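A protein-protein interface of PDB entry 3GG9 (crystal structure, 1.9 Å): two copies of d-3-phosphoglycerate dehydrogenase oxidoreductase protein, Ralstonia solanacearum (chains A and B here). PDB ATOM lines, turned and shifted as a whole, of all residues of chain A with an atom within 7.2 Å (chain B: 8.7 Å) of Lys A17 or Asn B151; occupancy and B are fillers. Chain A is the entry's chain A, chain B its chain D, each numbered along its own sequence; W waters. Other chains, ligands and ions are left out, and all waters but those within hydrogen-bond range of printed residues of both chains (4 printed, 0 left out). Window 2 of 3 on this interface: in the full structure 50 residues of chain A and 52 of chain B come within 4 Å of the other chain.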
ATOM      1  N   ASP A  10      21.714  -9.040  21.899  1.00  0.00           N
ATOM      2  CA  ASP A  10      21.067  -7.962  21.126  1.00  0.00           C
ATOM      3  C   ASP A  10      20.187  -8.566  20.027  1.00  0.00           C
ATOM      4  O   ASP A  10      20.606  -8.666  18.864  1.00  0.00           O
ATOM      5  CB  ASP A  10      22.136  -7.030  20.553  1.00  0.00           C
ATOM      6  CG  ASP A  10      21.558  -5.911  19.680  1.00  0.00           C
ATOM      7  OD1 ASP A  10      20.356  -5.571  19.794  1.00  0.00           O
ATOM      8  OD2 ASP A  10      22.335  -5.374  18.859  1.00  0.00           O
ATOM      9  N   GLN A  12      17.570  -7.932  18.165  1.00  0.00           N
ATOM     10  CA  GLN A  12      17.175  -7.266  16.928  1.00  0.00           C
ATOM     11  C   GLN A  12      18.330  -6.561  16.218  1.00  0.00           C
ATOM     12  O   GLN A  12      18.083  -5.767  15.304  1.00  0.00           O
ATOM     13  CB  GLN A  12      16.067  -6.249  17.214  1.00  0.00           C
ATOM     14  CG  GLN A  12      14.757  -6.900  17.494  1.00  0.00           C
ATOM     15  CD  GLN A  12      13.668  -5.943  17.954  1.00  0.00           C
ATOM     16  OE1 GLN A  12      13.593  -5.590  19.135  1.00  0.00           O
ATOM     17  NE2 GLN A  12      12.765  -5.578  17.029  1.00  0.00           N
ATOM     18  N   ASP A  13      19.561  -6.818  16.671  1.00  0.00           N
ATOM     19  CA  ASP A  13      20.790  -6.314  16.041  1.00  0.00           C
ATOM     20  C   ASP A  13      20.725  -4.795  15.943  1.00  0.00           C
ATOM     21  O   ASP A  13      21.009  -4.220  14.906  1.00  0.00           O
ATOM     22  CB  ASP A  13      20.969  -6.946  14.651  1.00  0.00           C
ATOM     23  CG  ASP A  13      22.399  -6.945  14.176  1.00  0.00           C
ATOM     24  OD1 ASP A  13      23.330  -6.830  15.018  1.00  0.00           O
ATOM     25  OD2 ASP A  13      22.577  -7.076  12.943  1.00  0.00           O
ATOM     26  N   ALA A  14      20.298  -4.150  17.023  1.00  0.00           N
ATOM     27  CA  ALA A  14      20.076  -2.699  17.003  1.00  0.00           C
ATOM     28  C   ALA A  14      21.298  -1.897  17.343  1.00  0.00           C
ATOM     29  O   ALA A  14      21.428  -0.756  16.905  1.00  0.00           O
ATOM     30  CB  ALA A  14      18.945  -2.314  17.977  1.00  0.00           C
ATOM     31  N   VAL A  15      22.150  -2.471  18.193  1.00  0.00           N
ATOM     32  CA  VAL A  15      23.298  -1.780  18.774  1.00  0.00           C
ATOM     33  C   VAL A  15      24.255  -1.251  17.710  1.00  0.00           C
ATOM     34  O   VAL A  15      24.682  -0.088  17.776  1.00  0.00           O
ATOM     35  CB  VAL A  15      24.053  -2.713  19.772  1.00  0.00           C
ATOM     36  CG1 VAL A  15      25.354  -2.080  20.272  1.00  0.00           C
ATOM     37  CG2 VAL A  15      23.117  -3.091  20.962  1.00  0.00           C
ATOM     38  N   ARG A  16      24.569  -2.090  16.719  1.00  0.00           N
ATOM     39  CA  ARG A  16      25.505  -1.691  15.675  1.00  0.00           C
ATOM     40  C   ARG A  16      24.978  -0.565  14.757  1.00  0.00           C
ATOM     41  O   ARG A  16      25.761   0.055  14.048  1.00  0.00           O
ATOM     42  CB  ARG A  16      26.020  -2.894  14.866  1.00  0.00           C
ATOM     43  CG  ARG A  16      25.046  -3.457  13.842  1.00  0.00           C
ATOM     44  CD  ARG A  16      25.687  -4.567  13.027  1.00  0.00           C
ATOM     45  NE  ARG A  16      24.687  -5.295  12.249  1.00  0.00           N
ATOM     46  CZ  ARG A  16      24.259  -4.955  11.033  1.00  0.00           C
ATOM     47  NH1 ARG A  16      24.741  -3.880  10.414  1.00  0.00           N
ATOM     48  NH2 ARG A  16      23.336  -5.696  10.430  1.00  0.00           N
ATOM     49  N   LYS A  17      23.671  -0.293  14.788  1.00  0.00           N
ATOM     50  CA  LYS A  17      23.107   0.784  13.966  1.00  0.00           C
ATOM     51  C   LYS A  17      22.918   2.092  14.720  1.00  0.00           C
ATOM     52  O   LYS A  17      22.417   3.056  14.153  1.00  0.00           O
ATOM     53  CB  LYS A  17      21.784   0.342  13.375  1.00  0.00           C
ATOM     54  CG  LYS A  17      21.901  -0.904  12.498  1.00  0.00           C
ATOM     55  CD  LYS A  17      20.559  -1.580  12.428  1.00  0.00           C
ATOM     56  CE  LYS A  17      20.639  -2.918  11.755  1.00  0.00           C
ATOM     57  NZ  LYS A  17      19.425  -3.682  12.131  1.00  0.00           N
ATOM     58  N   LEU A  18      23.307   2.131  15.992  1.00  0.00           N
ATOM     59  CA  LEU A  18      23.108   3.337  16.804  1.00  0.00           C
ATOM     60  C   LEU A  18      24.141   4.358  16.381  1.00  0.00           C
ATOM     61  O   LEU A  18      25.236   3.973  15.994  1.00  0.00           O
ATOM     62  CB  LEU A  18      23.285   3.034  18.294  1.00  0.00           C
ATOM     63  CG  LEU A  18      22.321   2.031  18.968  1.00  0.00           C
ATOM     64  CD1 LEU A  18      22.733   1.774  20.378  1.00  0.00           C
ATOM     65  CD2 LEU A  18      20.857   2.456  18.928  1.00  0.00           C
ATOM     66  N   ASP A  19      23.809   5.648  16.475  1.00  0.00           N
ATOM     67  CA  ASP A  19      24.796   6.709  16.257  1.00  0.00           C
ATOM     68  C   ASP A  19      26.013   6.539  17.156  1.00  0.00           C
ATOM     69  O   ASP A  19      27.135   6.769  16.722  1.00  0.00           O
ATOM     70  CB  ASP A  19      24.198   8.092  16.509  1.00  0.00           C
ATOM     71  CG  ASP A  19      23.134   8.483  15.473  1.00  0.00           C
ATOM     72  OD1 ASP A  19      23.016   7.828  14.411  1.00  0.00           O
ATOM     73  OD2 ASP A  19      22.397   9.452  15.737  1.00  0.00           O
ATOM     74  N   CYS A  20      25.787   6.105  18.400  1.00  0.00           N
ATOM     75  CA  CYS A  20      26.860   5.993  19.380  1.00  0.00           C
ATOM     76  C   CYS A  20      27.847   4.842  19.113  1.00  0.00           C
ATOM     77  O   CYS A  20      28.922   4.835  19.677  1.00  0.00           O
ATOM     78  CB  CYS A  20      26.295   5.913  20.809  1.00  0.00           C
ATOM     79  SG  CYS A  20      25.486   4.349  21.197  1.00  0.00           S
ATOM     80  N   PHE A  21      27.485   3.878  18.270  1.00  0.00           N
ATOM     81  CA  PHE A  21      28.379   2.760  17.949  1.00  0.00           C
ATOM     82  C   PHE A  21      29.757   3.202  17.416  1.00  0.00           C
ATOM     83  O   PHE A  21      30.758   2.488  17.592  1.00  0.00           O
ATOM     84  CB  PHE A  21      27.726   1.844  16.930  1.00  0.00           C
ATOM     85  CG  PHE A  21      28.362   0.496  16.848  1.00  0.00           C
ATOM     86  CD1 PHE A  21      28.191  -0.427  17.876  1.00  0.00           C
ATOM     87  CD2 PHE A  21      29.128   0.144  15.743  1.00  0.00           C
ATOM     88  CE1 PHE A  21      28.783  -1.686  17.801  1.00  0.00           C
ATOM     89  CE2 PHE A  21      29.729  -1.124  15.656  1.00  0.00           C
ATOM     90  CZ  PHE A  21      29.553  -2.031  16.677  1.00  0.00           C
ATOM     91  N   GLU A 305      14.113   0.764  23.171  1.00  0.00           N
ATOM     92  CA  GLU A 305      13.568   1.952  22.555  1.00  0.00           C
ATOM     93  C   GLU A 305      14.783   2.734  22.048  1.00  0.00           C
ATOM     94  O   GLU A 305      15.822   2.746  22.701  1.00  0.00           O
ATOM     95  CB  GLU A 305      12.746   2.738  23.590  1.00  0.00           C
ATOM     96  CG  GLU A 305      12.078   4.013  23.092  1.00  0.00           C
ATOM     97  CD  GLU A 305      12.985   5.228  23.087  1.00  0.00           C
ATOM     98  OE1 GLU A 305      13.680   5.465  24.108  1.00  0.00           O
ATOM     99  OE2 GLU A 305      12.991   5.963  22.065  1.00  0.00           O
ATOM    100  N   ARG A 306      14.634   3.411  20.921  1.00  0.00           N
ATOM    101  CA  ARG A 306      15.778   3.990  20.205  1.00  0.00           C
ATOM    102  C   ARG A 306      16.566   5.037  20.999  1.00  0.00           C
ATOM    103  O   ARG A 306      17.797   4.990  21.033  1.00  0.00           O
ATOM    104  CB  ARG A 306      15.353   4.531  18.833  1.00  0.00           C
ATOM    105  CG  ARG A 306      14.145   5.445  18.850  1.00  0.00           C
ATOM    106  CD  ARG A 306      14.357   6.561  17.862  1.00  0.00           C
ATOM    107  NE  ARG A 306      13.595   7.763  18.189  1.00  0.00           N
ATOM    108  CZ  ARG A 306      14.066   8.993  18.014  1.00  0.00           C
ATOM    109  NH1 ARG A 306      15.297   9.170  17.544  1.00  0.00           N
ATOM    110  NH2 ARG A 306      13.321  10.048  18.328  1.00  0.00           N
ATOM    111  N   TYR A 309      18.283   3.289  23.988  1.00  0.00           N
ATOM    112  CA  TYR A 309      19.511   2.594  23.540  1.00  0.00           C
ATOM    113  C   TYR A 309      20.653   3.601  23.254  1.00  0.00           C
ATOM    114  O   TYR A 309      21.795   3.421  23.688  1.00  0.00           O
ATOM    115  CB  TYR A 309      19.218   1.734  22.302  1.00  0.00           C
ATOM    116  CG  TYR A 309      18.861   0.264  22.607  1.00  0.00           C
ATOM    117  CD1 TYR A 309      18.232  -0.101  23.804  1.00  0.00           C
ATOM    118  CD2 TYR A 309      19.133  -0.748  21.681  1.00  0.00           C
ATOM    119  CE1 TYR A 309      17.909  -1.456  24.086  1.00  0.00           C
ATOM    120  CE2 TYR A 309      18.818  -2.104  21.963  1.00  0.00           C
ATOM    121  CZ  TYR A 309      18.206  -2.437  23.170  1.00  0.00           C
ATOM    122  OH  TYR A 309      17.872  -3.758  23.467  1.00  0.00           O
ATOM    123  N   GLU A 310      20.336   4.680  22.557  1.00  0.00           N
ATOM    124  CA  GLU A 310      21.355   5.699  22.303  1.00  0.00           C
ATOM    125  C   GLU A 310      22.020   6.154  23.613  1.00  0.00           C
ATOM    126  O   GLU A 310      23.240   6.142  23.699  1.00  0.00           O
ATOM    127  CB  GLU A 310      20.794   6.895  21.513  1.00  0.00           C
ATOM    128  CG  GLU A 310      20.459   6.609  20.031  1.00  0.00           C
ATOM    129  CD  GLU A 310      21.670   6.402  19.093  1.00  0.00           C
ATOM    130  OE1 GLU A 310      21.404   6.141  17.884  1.00  0.00           O
ATOM    131  OE2 GLU A 310      22.866   6.490  19.528  1.00  0.00           O
ATOM    132  N   GLN B 123       3.707   3.163  18.261  1.00  0.00           N
ATOM    133  CA  GLN B 123       5.068   3.599  18.574  1.00  0.00           C
ATOM    134  C   GLN B 123       5.924   2.605  19.346  1.00  0.00           C
ATOM    135  O   GLN B 123       7.137   2.647  19.243  1.00  0.00           O
ATOM    136  CB  GLN B 123       5.090   4.985  19.254  1.00  0.00           C
ATOM    137  CG  GLN B 123       4.516   6.063  18.388  1.00  0.00           C
ATOM    138  CD  GLN B 123       5.325   6.304  17.129  1.00  0.00           C
ATOM    139  OE1 GLN B 123       5.158   5.620  16.120  1.00  0.00           O
ATOM    140  NE2 GLN B 123       6.198   7.282  17.179  1.00  0.00           N
ATOM    141  N   ARG B 125       5.304  -0.761  18.863  1.00  0.00           N
ATOM    142  CA  ARG B 125       5.212  -1.955  17.996  1.00  0.00           C
ATOM    143  C   ARG B 125       4.639  -3.147  18.777  1.00  0.00           C
ATOM    144  O   ARG B 125       5.017  -4.296  18.550  1.00  0.00           O
ATOM    145  CB  ARG B 125       6.564  -2.295  17.343  1.00  0.00           C
ATOM    146  CG  ARG B 125       7.033  -1.329  16.225  1.00  0.00           C
ATOM    147  CD  ARG B 125       7.718  -0.107  16.775  1.00  0.00           C
ATOM    148  NE  ARG B 125       8.433   0.713  15.789  1.00  0.00           N
ATOM    149  CZ  ARG B 125       8.008   1.880  15.304  1.00  0.00           C
ATOM    150  NH1 ARG B 125       8.767   2.540  14.428  1.00  0.00           N
ATOM    151  NH2 ARG B 125       6.835   2.392  15.673  1.00  0.00           N
ATOM    152  N   TYR B 129       5.230  -7.159  18.373  1.00  0.00           N
ATOM    153  CA  TYR B 129       6.018  -7.862  19.400  1.00  0.00           C
ATOM    154  C   TYR B 129       5.197  -8.970  20.054  1.00  0.00           C
ATOM    155  O   TYR B 129       5.712 -10.054  20.293  1.00  0.00           O
ATOM    156  CB  TYR B 129       6.523  -6.909  20.472  1.00  0.00           C
ATOM    157  CG  TYR B 129       7.836  -6.210  20.202  1.00  0.00           C
ATOM    158  CD1 TYR B 129       9.014  -6.927  20.007  1.00  0.00           C
ATOM    159  CD2 TYR B 129       7.895  -4.806  20.172  1.00  0.00           C
ATOM    160  CE1 TYR B 129      10.216  -6.278  19.785  1.00  0.00           C
ATOM    161  CE2 TYR B 129       9.087  -4.150  19.939  1.00  0.00           C
ATOM    162  CZ  TYR B 129      10.237  -4.871  19.752  1.00  0.00           C
ATOM    163  OH  TYR B 129      11.411  -4.187  19.572  1.00  0.00           O
ATOM    164  N   SER B 141       9.895  -7.596  16.382  1.00  0.00           N
ATOM    165  CA  SER B 141       8.680  -6.932  15.947  1.00  0.00           C
ATOM    166  C   SER B 141       8.362  -7.400  14.524  1.00  0.00           C
ATOM    167  O   SER B 141       7.220  -7.324  14.076  1.00  0.00           O
ATOM    168  CB  SER B 141       8.825  -5.422  16.033  1.00  0.00           C
ATOM    169  OG  SER B 141       9.929  -4.991  15.263  1.00  0.00           O
ATOM    170  N   LEU B 143       9.421  -6.186  11.684  1.00  0.00           N
ATOM    171  CA  LEU B 143       9.443  -5.154  10.665  1.00  0.00           C
ATOM    172  C   LEU B 143      10.712  -5.396   9.868  1.00  0.00           C
ATOM    173  O   LEU B 143      11.787  -4.883  10.195  1.00  0.00           O
ATOM    174  CB  LEU B 143       9.390  -3.746  11.276  1.00  0.00           C
ATOM    175  CG  LEU B 143       8.029  -3.200  11.742  1.00  0.00           C
ATOM    176  CD1 LEU B 143       8.217  -1.999  12.644  1.00  0.00           C
ATOM    177  CD2 LEU B 143       7.126  -2.814  10.574  1.00  0.00           C
ATOM    178  N   SER B 145      11.434  -4.946   6.486  1.00  0.00           N
ATOM    179  CA  SER B 145      11.730  -4.213   5.248  1.00  0.00           C
ATOM    180  C   SER B 145      13.161  -3.679   5.217  1.00  0.00           C
ATOM    181  O   SER B 145      13.744  -3.354   6.252  1.00  0.00           O
ATOM    182  CB  SER B 145      10.709  -3.102   4.991  1.00  0.00           C
ATOM    183  OG  SER B 145      11.205  -2.127   4.085  1.00  0.00           O
ATOM    184  N   MET B 148      13.302   0.539   5.294  1.00  0.00           N
ATOM    185  CA  MET B 148      12.905   1.283   6.507  1.00  0.00           C
ATOM    186  C   MET B 148      14.095   2.005   7.159  1.00  0.00           C
ATOM    187  O   MET B 148      15.237   1.586   6.971  1.00  0.00           O
ATOM    188  CB  MET B 148      12.288   0.327   7.517  1.00  0.00           C
ATOM    189  CG  MET B 148      11.012  -0.292   7.029  1.00  0.00           C
ATOM    190  SD  MET B 148      10.317  -1.439   8.214  1.00  0.00           S
ATOM    191  CE  MET B 148      11.723  -1.784   9.255  1.00  0.00           C
ATOM    192  N   PRO B 149      13.845   3.098   7.928  1.00  0.00           N
ATOM    193  CA  PRO B 149      14.950   3.699   8.693  1.00  0.00           C
ATOM    194  C   PRO B 149      15.638   2.669   9.613  1.00  0.00           C
ATOM    195  O   PRO B 149      14.998   1.681   9.999  1.00  0.00           O
ATOM    196  CB  PRO B 149      14.250   4.788   9.514  1.00  0.00           C
ATOM    197  CG  PRO B 149      13.082   5.148   8.712  1.00  0.00           C
ATOM    198  CD  PRO B 149      12.597   3.859   8.121  1.00  0.00           C
ATOM    199  N   PRO B 150      16.935   2.877   9.931  1.00  0.00           N
ATOM    200  CA  PRO B 150      17.673   1.980  10.823  1.00  0.00           C
ATOM    201  C   PRO B 150      16.987   1.902  12.175  1.00  0.00           C
ATOM    202  O   PRO B 150      16.557   2.927  12.718  1.00  0.00           O
ATOM    203  CB  PRO B 150      19.035   2.675  10.976  1.00  0.00           C
ATOM    204  CG  PRO B 150      18.777   4.111  10.609  1.00  0.00           C
ATOM    205  CD  PRO B 150      17.786   3.999   9.486  1.00  0.00           C
ATOM    206  N   ASN B 151      16.851   0.682  12.687  1.00  0.00           N
ATOM    207  CA  ASN B 151      16.192   0.438  13.978  1.00  0.00           C
ATOM    208  C   ASN B 151      14.702   0.807  14.065  1.00  0.00           C
ATOM    209  O   ASN B 151      14.145   0.963  15.163  1.00  0.00           O
ATOM    210  CB  ASN B 151      16.989   1.051  15.130  1.00  0.00           C
ATOM    211  CG  ASN B 151      18.231   0.279  15.439  1.00  0.00           C
ATOM    212  OD1 ASN B 151      18.397  -0.867  14.996  1.00  0.00           O
ATOM    213  ND2 ASN B 151      19.131   0.899  16.177  1.00  0.00           N
ATOM    214  N   PHE B 152      14.038   0.888  12.919  1.00  0.00           N
ATOM    215  CA  PHE B 152      12.610   1.207  12.908  1.00  0.00           C
ATOM    216  C   PHE B 152      11.782   0.086  13.578  1.00  0.00           C
ATOM    217  O   PHE B 152      10.696   0.325  14.062  1.00  0.00           O
ATOM    218  CB  PHE B 152      12.133   1.435  11.472  1.00  0.00           C
ATOM    219  CG  PHE B 152      10.875   2.256  11.378  1.00  0.00           C
ATOM    220  CD1 PHE B 152      10.833   3.546  11.915  1.00  0.00           C
ATOM    221  CD2 PHE B 152       9.748   1.754  10.755  1.00  0.00           C
ATOM    222  CE1 PHE B 152       9.683   4.305  11.834  1.00  0.00           C
ATOM    223  CE2 PHE B 152       8.597   2.503  10.669  1.00  0.00           C
ATOM    224  CZ  PHE B 152       8.568   3.791  11.213  1.00  0.00           C
ATOM    225  N   GLY B 153      12.325  -1.123  13.644  1.00  0.00           N
ATOM    226  CA  GLY B 153      11.614  -2.210  14.328  1.00  0.00           C
ATOM    227  C   GLY B 153      11.597  -2.111  15.853  1.00  0.00           C
ATOM    228  O   GLY B 153      10.866  -2.861  16.507  1.00  0.00           O
ATOM    229  N   ILE B 154      12.394  -1.209  16.445  1.00  0.00           N
ATOM    230  CA  ILE B 154      12.305  -1.022  17.891  1.00  0.00           C
ATOM    231  C   ILE B 154      11.442   0.208  18.242  1.00  0.00           C
ATOM    232  O   ILE B 154      11.200   1.063  17.387  1.00  0.00           O
ATOM    233  CB  ILE B 154      13.694  -1.037  18.628  1.00  0.00           C
ATOM    234  CG1 ILE B 154      14.461   0.272  18.424  1.00  0.00           C
ATOM    235  CG2 ILE B 154      14.552  -2.290  18.219  1.00  0.00           C
ATOM    236  CD1 ILE B 154      15.786   0.326  19.152  1.00  0.00           C
ATOM    237  N   GLY B 155      10.987   0.271  19.491  1.00  0.00           N
ATOM    238  CA  GLY B 155      10.043   1.299  19.948  1.00  0.00           C
ATOM    239  C   GLY B 155      10.645   2.691  19.943  1.00  0.00           C
ATOM    240  O   GLY B 155      11.851   2.862  19.753  1.00  0.00           O
ATOM    241  N   ARG B 156       9.789   3.693  20.141  1.00  0.00           N
ATOM    242  CA  ARG B 156      10.178   5.100  20.045  1.00  0.00           C
ATOM    243  C   ARG B 156       9.445   5.816  21.176  1.00  0.00           C
ATOM    244  O   ARG B 156       8.235   5.639  21.317  1.00  0.00           O
ATOM    245  CB  ARG B 156       9.746   5.679  18.691  1.00  0.00           C
ATOM    246  CG  ARG B 156      10.382   5.000  17.478  1.00  0.00           C
ATOM    247  CD  ARG B 156      10.005   5.627  16.152  1.00  0.00           C
ATOM    248  NE  ARG B 156      10.809   6.810  15.823  1.00  0.00           N
ATOM    249  CZ  ARG B 156      11.996   6.778  15.217  1.00  0.00           C
ATOM    250  NH1 ARG B 156      12.563   5.615  14.898  1.00  0.00           N
ATOM    251  NH2 ARG B 156      12.634   7.912  14.942  1.00  0.00           N
ATOM    252  N   THR B 244      10.214   8.208   9.205  1.00  0.00           N
ATOM    253  CA  THR B 244      10.109   7.719  10.593  1.00  0.00           C
ATOM    254  C   THR B 244       8.743   7.992  11.247  1.00  0.00           C
ATOM    255  O   THR B 244       8.470   7.513  12.363  1.00  0.00           O
ATOM    256  CB  THR B 244      11.173   8.365  11.522  1.00  0.00           C
ATOM    257  OG1 THR B 244      11.107   9.805  11.408  1.00  0.00           O
ATOM    258  CG2 THR B 244      12.559   7.911  11.144  1.00  0.00           C
HETATM  259  O   HOH W   1      17.134  -3.190  14.819  1.00  0.00           O
HETATM  260  O   HOH W   2      13.018  -5.643  14.079  1.00  0.00           O
HETATM  261  O   HOH W   3      17.089  -1.585  11.334  1.00  0.00           O
HETATM  262  O   HOH W   4      11.976  10.687  15.206  1.00  0.00           O
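O of Ala A14 is in hydrogen-bond range of ND2 of Asn B151, 2.9 Å away.
NE of Arg A306 sits close to NH2 of Arg B156 (3.4 Å).
The backbone carbonyl oxygen (O) of Gly B155 sits at hydrogen-bond distance from the backbone NH (N) of Arg A306, 3.1 Å away.
The side-chain amide oxygen (OE1) of Gln A12 is in hydrogen-bond range of the side-chain hydroxyl (OH) of Tyr B129, at 2.6 Å.
The side-chain amide nitrogen of Gln A12 lies within hydrogen-bond range of the side-chain hydroxyl of Ser B141 (3.4 Å).
O of Gly B153 sits at hydrogen-bond distance from NE2 of Gln A12.
The side-chain hydroxyl (OG) of Ser B141 lies within hydrogen-bond range of the backbone carbonyl oxygen (O) of Gly B153, at 2.6 Å.
N of Arg B156 sits at hydrogen-bond distance from O of Gln B123 (3.0 Å).
The side-chain amino group (NZ) of Lys A17 sits at hydrogen-bond distance from the backbone carbonyl oxygen (O) of Asp A13.
N of Ala A14 is in hydrogen-bond range of OD2 of Asp A10, 3.0 Å away.
The side-chain hydroxyl (OH) of Tyr B129 is in hydrogen-bond range of the backbone carbonyl oxygen (O) of Gly B153, 3.4 Å away.
The backbone carbonyl oxygen (O) of Ile B154 lies within hydrogen-bond range of the guanidinium group (NE) of Arg B125, 3.2 Å away.
Gln A12 touches Ile B154.
Asn B151 touches Lys A17.
CD2 of Leu A18 touches ND2 of Asn B151, 3.6 Å away.
Glu A305 touches Ile B154 (C to CD1, 3.9 Å).
O of Gly B155 touches CA of Glu A305, 3.4 Å away.
OE2 of Glu A305 touches CA of Arg B156 (3.6 Å).
CD1 of Ile B154 touches N of Arg A306, 3.7 Å away.
Of chain B, only Asn B151 comes within 4 Å of Lys A17.
Asn B151 touches just these residues of chain A: Ala A14 (2.9 Å), Lys A17 (3.4 Å) and Leu A18 (3.6 Å).
Printed residues of chain B within 4 Å of Ala A14: Asn B151 (2.9 Å).
Of the printed residues of chain B, Leu A18 touches Asn B151.
Of the printed residues of chain A, Ser B141 touches Gln A12.
Of the printed residues of chain A, Arg B156 touches Glu A305 (3.6 Å) and Arg A306 (3.4 Å).
Printed residues of chain A within 4 Å of Gly B153: Gln A12 (3.4 Å).
Asp A13 touches none of the printed residues of chain B.
The nearest printed residue of chain B that does not touch Glu A305 is Gln B123 (6.4 Å).
Of the 16 printed residues of chain B, 7 touch a printed residue of chain A.
No position is printed for both chains.
Water W1 lies within hydrogen-bond range of OD1 of Asn B151 (2.7 Å) and O of Gln A12 (2.8 Å).
Water W3 bridges N of Asn B151 (2.7 Å) and NZ of Lys A17 (3.2 Å).
Water W4 lies within hydrogen-bond range of NH2 of Arg B156 (2.9 Å) and NH2 of Arg A306 (3.5 Å).
Water W2 bridges NE2 of Gln A12 and OG of Ser B141.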
